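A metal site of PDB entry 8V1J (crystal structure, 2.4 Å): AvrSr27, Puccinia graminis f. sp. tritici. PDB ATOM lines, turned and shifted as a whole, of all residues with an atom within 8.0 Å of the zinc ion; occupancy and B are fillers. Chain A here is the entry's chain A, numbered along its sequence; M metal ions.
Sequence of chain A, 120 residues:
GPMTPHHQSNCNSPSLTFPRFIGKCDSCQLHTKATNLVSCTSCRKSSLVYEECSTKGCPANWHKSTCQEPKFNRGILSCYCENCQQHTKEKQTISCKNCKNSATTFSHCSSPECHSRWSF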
ATOM      1  N   ASN A  61     -12.879  -9.165 -15.291  1.00  0.00           N
ATOM      2  CA  ASN A  61     -11.823  -9.229 -16.287  1.00  0.00           C
ATOM      3  C   ASN A  61     -12.386  -9.878 -17.541  1.00  0.00           C
ATOM      4  O   ASN A  61     -12.863 -11.020 -17.492  1.00  0.00           O
ATOM      5  CB  ASN A  61     -10.622 -10.009 -15.740  1.00  0.00           C
ATOM      6  CG  ASN A  61      -9.452 -10.044 -16.715  1.00  0.00           C
ATOM      7  OD1 ASN A  61      -9.602  -9.830 -17.918  1.00  0.00           O
ATOM      8  ND2 ASN A  61      -8.269 -10.318 -16.185  1.00  0.00           N
ATOM      9  N   TRP A  62     -12.330  -9.164 -18.666  1.00  0.00           N
ATOM     10  CA  TRP A  62     -13.006  -9.581 -19.895  1.00  0.00           C
ATOM     11  C   TRP A  62     -12.196 -10.561 -20.724  1.00  0.00           C
ATOM     12  O   TRP A  62     -12.665 -10.955 -21.804  1.00  0.00           O
ATOM     13  CB  TRP A  62     -13.366  -8.349 -20.733  1.00  0.00           C
ATOM     14  CG  TRP A  62     -12.215  -7.415 -20.975  1.00  0.00           C
ATOM     15  CD1 TRP A  62     -11.852  -6.342 -20.209  1.00  0.00           C
ATOM     16  CD2 TRP A  62     -11.279  -7.460 -22.058  1.00  0.00           C
ATOM     17  NE1 TRP A  62     -10.740  -5.725 -20.743  1.00  0.00           N
ATOM     18  CE2 TRP A  62     -10.376  -6.390 -21.885  1.00  0.00           C
ATOM     19  CE3 TRP A  62     -11.115  -8.300 -23.166  1.00  0.00           C
ATOM     20  CZ2 TRP A  62      -9.326  -6.148 -22.768  1.00  0.00           C
ATOM     21  CZ3 TRP A  62     -10.075  -8.047 -24.048  1.00  0.00           C
ATOM     22  CH2 TRP A  62      -9.198  -6.981 -23.838  1.00  0.00           C
ATOM     23  N   HIS A  63     -11.020 -10.978 -20.272  1.00  0.00           N
ATOM     24  CA  HIS A  63     -10.203 -11.931 -21.010  1.00  0.00           C
ATOM     25  C   HIS A  63     -10.670 -13.354 -20.754  1.00  0.00           C
ATOM     26  O   HIS A  63     -11.209 -13.683 -19.697  1.00  0.00           O
ATOM     27  CB  HIS A  63      -8.733 -11.805 -20.605  1.00  0.00           C
ATOM     28  CG  HIS A  63      -8.077 -10.542 -21.066  1.00  0.00           C
ATOM     29  ND1 HIS A  63      -7.344 -10.470 -22.235  1.00  0.00           N
ATOM     30  CD2 HIS A  63      -8.029  -9.307 -20.509  1.00  0.00           C
ATOM     31  CE1 HIS A  63      -6.880  -9.237 -22.378  1.00  0.00           C
ATOM     32  NE2 HIS A  63      -7.287  -8.520 -21.348  1.00  0.00           N
ATOM     33  N   LYS A  64     -10.449 -14.208 -21.759  1.00  0.00           N
ATOM     34  CA  LYS A  64     -10.699 -15.637 -21.575  1.00  0.00           C
ATOM     35  C   LYS A  64      -9.898 -16.163 -20.393  1.00  0.00           C
ATOM     36  O   LYS A  64      -8.884 -15.599 -19.992  1.00  0.00           O
ATOM     37  CB  LYS A  64     -10.311 -16.411 -22.833  1.00  0.00           C
ATOM     38  CG  LYS A  64     -11.263 -16.260 -24.005  1.00  0.00           C
ATOM     39  CD  LYS A  64     -10.768 -17.055 -25.203  1.00  0.00           C
ATOM     40  CE  LYS A  64     -11.791 -17.090 -26.323  1.00  0.00           C
ATOM     41  NZ  LYS A  64     -11.341 -16.347 -27.533  1.00  0.00           N
ATOM     42  N   SER A  65     -10.369 -17.283 -19.844  1.00  0.00           N
ATOM     43  CA  SER A  65      -9.623 -17.951 -18.784  1.00  0.00           C
ATOM     44  C   SER A  65      -8.315 -18.534 -19.279  1.00  0.00           C
ATOM     45  O   SER A  65      -7.393 -18.728 -18.484  1.00  0.00           O
ATOM     46  CB  SER A  65     -10.487 -19.056 -18.162  1.00  0.00           C
ATOM     47  OG  SER A  65     -11.142 -19.816 -19.165  1.00  0.00           O
ATOM     48  N   THR A  66      -8.202 -18.807 -20.584  1.00  0.00           N
ATOM     49  CA  THR A  66      -7.006 -19.399 -21.171  1.00  0.00           C
ATOM     50  C   THR A  66      -6.023 -18.350 -21.700  1.00  0.00           C
ATOM     51  O   THR A  66      -5.016 -18.720 -22.307  1.00  0.00           O
ATOM     52  CB  THR A  66      -7.406 -20.345 -22.307  1.00  0.00           C
ATOM     53  OG1 THR A  66      -8.299 -19.678 -23.204  1.00  0.00           O
ATOM     54  CG2 THR A  66      -8.083 -21.582 -21.749  1.00  0.00           C
ATOM     55  N   CYS A  67      -6.297 -17.067 -21.478  1.00  0.00           N
ATOM     56  CA  CYS A  67      -5.422 -16.019 -21.998  1.00  0.00           C
ATOM     57  C   CYS A  67      -4.093 -16.035 -21.266  1.00  0.00           C
ATOM     58  O   CYS A  67      -4.054 -15.876 -20.036  1.00  0.00           O
ATOM     59  CB  CYS A  67      -6.101 -14.653 -21.856  1.00  0.00           C
ATOM     60  SG  CYS A  67      -5.074 -13.263 -22.423  1.00  0.00           S
ATOM     61  N   GLN A  68      -3.002 -16.224 -22.012  1.00  0.00           N
ATOM     62  CA  GLN A  68      -1.672 -16.252 -21.416  1.00  0.00           C
ATOM     63  C   GLN A  68      -1.166 -14.847 -21.120  1.00  0.00           C
ATOM     64  O   GLN A  68      -0.537 -14.616 -20.080  1.00  0.00           O
ATOM     65  CB  GLN A  68      -0.687 -16.950 -22.367  1.00  0.00           C
ATOM     66  CG  GLN A  68      -1.211 -18.187 -23.086  1.00  0.00           C
ATOM     67  CD  GLN A  68      -0.337 -18.555 -24.274  1.00  0.00           C
ATOM     68  OE1 GLN A  68       0.279 -17.685 -24.894  1.00  0.00           O
ATOM     69  NE2 GLN A  68      -0.289 -19.842 -24.600  1.00  0.00           N
ATOM     70  N   GLU A  69      -1.407 -13.901 -22.030  1.00  0.00           N
ATOM     71  CA  GLU A  69      -0.863 -12.550 -21.916  1.00  0.00           C
ATOM     72  C   GLU A  69      -1.814 -11.531 -22.538  1.00  0.00           C
ATOM     73  O   GLU A  69      -2.058 -11.579 -23.750  1.00  0.00           O
ATOM     74  CB  GLU A  69       0.491 -12.459 -22.619  1.00  0.00           C
ATOM     75  CG  GLU A  69       1.680 -12.803 -21.737  1.00  0.00           C
ATOM     76  CD  GLU A  69       2.959 -12.178 -22.248  1.00  0.00           C
ATOM     77  OE1 GLU A  69       3.067 -11.949 -23.470  1.00  0.00           O
ATOM     78  OE2 GLU A  69       3.859 -11.908 -21.420  1.00  0.00           O
ATOM     79  N   PRO A  70      -2.367 -10.605 -21.760  1.00  0.00           N
ATOM     80  CA  PRO A  70      -3.155  -9.521 -22.354  1.00  0.00           C
ATOM     81  C   PRO A  70      -2.354  -8.737 -23.387  1.00  0.00           C
ATOM     82  O   PRO A  70      -1.373  -8.073 -23.047  1.00  0.00           O
ATOM     83  CB  PRO A  70      -3.516  -8.645 -21.148  1.00  0.00           C
ATOM     84  CG  PRO A  70      -3.514  -9.581 -19.999  1.00  0.00           C
ATOM     85  CD  PRO A  70      -2.431 -10.592 -20.284  1.00  0.00           C
ATOM     86  N   LYS A  71      -2.771  -8.821 -24.653  1.00  0.00           N
ATOM     87  CA  LYS A  71      -2.159  -8.051 -25.740  1.00  0.00           C
ATOM     88  C   LYS A  71      -3.178  -6.984 -26.159  1.00  0.00           C
ATOM     89  O   LYS A  71      -4.008  -7.211 -27.041  1.00  0.00           O
ATOM     90  CB  LYS A  71      -1.757  -8.950 -26.910  1.00  0.00           C
ATOM     91  CG  LYS A  71      -0.351  -9.528 -26.788  1.00  0.00           C
ATOM     92  CD  LYS A  71       0.224  -9.898 -28.159  1.00  0.00           C
ATOM     93  CE  LYS A  71      -0.432 -11.140 -28.742  1.00  0.00           C
ATOM     94  NZ  LYS A  71      -0.308 -11.196 -30.226  1.00  0.00           N
ATOM     95  N   PHE A  72      -3.085  -5.825 -25.518  1.00  0.00           N
ATOM     96  CA  PHE A  72      -4.096  -4.781 -25.641  1.00  0.00           C
ATOM     97  C   PHE A  72      -3.981  -4.059 -26.980  1.00  0.00           C
ATOM     98  O   PHE A  72      -2.893  -3.649 -27.381  1.00  0.00           O
ATOM     99  CB  PHE A  72      -3.927  -3.804 -24.475  1.00  0.00           C
ATOM    100  CG  PHE A  72      -5.085  -2.871 -24.280  1.00  0.00           C
ATOM    101  CD1 PHE A  72      -5.054  -1.582 -24.815  1.00  0.00           C
ATOM    102  CD2 PHE A  72      -6.180  -3.255 -23.538  1.00  0.00           C
ATOM    103  CE1 PHE A  72      -6.110  -0.716 -24.624  1.00  0.00           C
ATOM    104  CE2 PHE A  72      -7.242  -2.384 -23.340  1.00  0.00           C
ATOM    105  CZ  PHE A  72      -7.205  -1.116 -23.886  1.00  0.00           C
ATOM    106  N   SER A  95     -10.080  -5.124 -27.506  1.00  0.00           N
ATOM    107  CA  SER A  95      -9.960  -6.567 -27.647  1.00  0.00           C
ATOM    108  C   SER A  95      -8.523  -6.986 -27.405  1.00  0.00           C
ATOM    109  O   SER A  95      -7.609  -6.159 -27.337  1.00  0.00           O
ATOM    110  CB  SER A  95     -10.451  -7.026 -29.025  1.00  0.00           C
ATOM    111  OG  SER A  95      -9.779  -6.337 -30.055  1.00  0.00           O
ATOM    112  N   CYS A  96      -8.328  -8.296 -27.272  1.00  0.00           N
ATOM    113  CA  CYS A  96      -7.024  -8.885 -26.984  1.00  0.00           C
ATOM    114  C   CYS A  96      -6.539  -9.651 -28.207  1.00  0.00           C
ATOM    115  O   CYS A  96      -7.269 -10.492 -28.747  1.00  0.00           O
ATOM    116  CB  CYS A  96      -7.125  -9.820 -25.779  1.00  0.00           C
ATOM    117  SG  CYS A  96      -5.576 -10.587 -25.273  1.00  0.00           S
ATOM    118  N   LYS A  97      -5.318  -9.352 -28.643  1.00  0.00           N
ATOM    119  CA  LYS A  97      -4.789  -9.990 -29.849  1.00  0.00           C
ATOM    120  C   LYS A  97      -4.496 -11.469 -29.631  1.00  0.00           C
ATOM    121  O   LYS A  97      -4.532 -12.251 -30.582  1.00  0.00           O
ATOM    122  CB  LYS A  97      -3.523  -9.263 -30.317  1.00  0.00           C
ATOM    123  CG  LYS A  97      -3.786  -7.881 -30.901  1.00  0.00           C
ATOM    124  CD  LYS A  97      -2.537  -7.300 -31.542  1.00  0.00           C
ATOM    125  CE  LYS A  97      -2.862  -6.076 -32.388  1.00  0.00           C
ATOM    126  NZ  LYS A  97      -1.642  -5.474 -32.995  1.00  0.00           N
ATOM    127  N   ASN A  98      -4.187 -11.866 -28.399  1.00  0.00           N
ATOM    128  CA  ASN A  98      -3.887 -13.262 -28.123  1.00  0.00           C
ATOM    129  C   ASN A  98      -5.164 -14.069 -27.892  1.00  0.00           C
ATOM    130  O   ASN A  98      -5.376 -15.105 -28.521  1.00  0.00           O
ATOM    131  CB  ASN A  98      -2.946 -13.378 -26.923  1.00  0.00           C
ATOM    132  CG  ASN A  98      -2.870 -14.792 -26.365  1.00  0.00           C
ATOM    133  OD1 ASN A  98      -3.022 -15.772 -27.108  1.00  0.00           O
ATOM    134  ND2 ASN A  98      -2.651 -14.907 -25.062  1.00  0.00           N
ATOM    135  N   CYS A  99      -6.030 -13.597 -26.992  1.00  0.00           N
ATOM    136  CA  CYS A  99      -7.149 -14.401 -26.525  1.00  0.00           C
ATOM    137  C   CYS A  99      -8.448 -14.143 -27.277  1.00  0.00           C
ATOM    138  O   CYS A  99      -9.351 -14.983 -27.226  1.00  0.00           O
ATOM    139  CB  CYS A  99      -7.349 -14.182 -25.016  1.00  0.00           C
ATOM    140  SG  CYS A  99      -8.494 -12.871 -24.573  1.00  0.00           S
ATOM    141  N   LYS A 100      -8.563 -13.008 -27.976  1.00  0.00           N
ATOM    142  CA  LYS A 100      -9.639 -12.710 -28.922  1.00  0.00           C
ATOM    143  C   LYS A 100     -10.936 -12.239 -28.262  1.00  0.00           C
ATOM    144  O   LYS A 100     -11.903 -11.975 -28.979  1.00  0.00           O
ATOM    145  CB  LYS A 100      -9.978 -13.918 -29.818  1.00  0.00           C
ATOM    146  CG  LYS A 100      -8.778 -14.584 -30.473  1.00  0.00           C
ATOM    147  CD  LYS A 100      -8.085 -13.653 -31.441  1.00  0.00           C
ATOM    148  CE  LYS A 100      -7.032 -14.394 -32.264  1.00  0.00           C
ATOM    149  NZ  LYS A 100      -6.719 -13.696 -33.535  1.00  0.00           N
ATOM    150  N   ASN A 101     -10.990 -12.134 -26.935  1.00  0.00           N
ATOM    151  CA  ASN A 101     -12.166 -11.573 -26.283  1.00  0.00           C
ATOM    152  C   ASN A 101     -12.151 -10.049 -26.381  1.00  0.00           C
ATOM    153  O   ASN A 101     -11.149  -9.431 -26.749  1.00  0.00           O
ATOM    154  CB  ASN A 101     -12.231 -12.008 -24.813  1.00  0.00           C
ATOM    155  CG  ASN A 101     -13.005 -13.296 -24.613  1.00  0.00           C
ATOM    156  OD1 ASN A 101     -13.231 -14.059 -25.550  1.00  0.00           O
ATOM    157  ND2 ASN A 101     -13.424 -13.535 -23.378  1.00  0.00           N
ATOM    158  N   SER A 102     -13.281  -9.443 -26.036  1.00  0.00           N
ATOM    159  CA  SER A 102     -13.441  -8.005 -26.100  1.00  0.00           C
ATOM    160  C   SER A 102     -14.092  -7.494 -24.821  1.00  0.00           C
ATOM    161  O   SER A 102     -14.770  -8.238 -24.113  1.00  0.00           O
ATOM    162  CB  SER A 102     -14.277  -7.591 -27.317  1.00  0.00           C
ATOM    163  OG  SER A 102     -13.661  -7.990 -28.520  1.00  0.00           O
HETATM  164 ZN    ZN M   1      -6.574 -11.849 -23.554  1.00  0.00          ZN
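The backbone NH (N) of His 63 is in hydrogen-bond range of the side-chain amide oxygen (OD1) of Asn 61, at 3.0 Å.
The side-chain sulfur (SG) of Cys 67 lies close to the backbone carbonyl oxygen (O) of Glu 69, at 3.7 Å.
The side-chain sulfur (SG) of Cys 96 sits close to the backbone NH (N) of Lys 71, at 3.4 Å.
The side-chain sulfur (SG) of Cys 96 sits close to the backbone NH (N) of Asn 98, at 3.7 Å.
N of Cys 96 is in hydrogen-bond range of O of Asn 101, at 3.1 Å.
The backbone carbonyl oxygen (O) of Cys 99 is in hydrogen-bond range of the side-chain amino group (NZ) of Lys 64, 2.4 Å away.
The side-chain sulfur (SG) of Cys 99 lies close to the backbone NH (N) of Asn 101 (3.5 Å).
The zinc ion is bound by ND1 of His 63, SG of Cys 67, SG of Cys 96 and SG of Cys 99.
The zinc ion has four donor atoms within binding distance.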
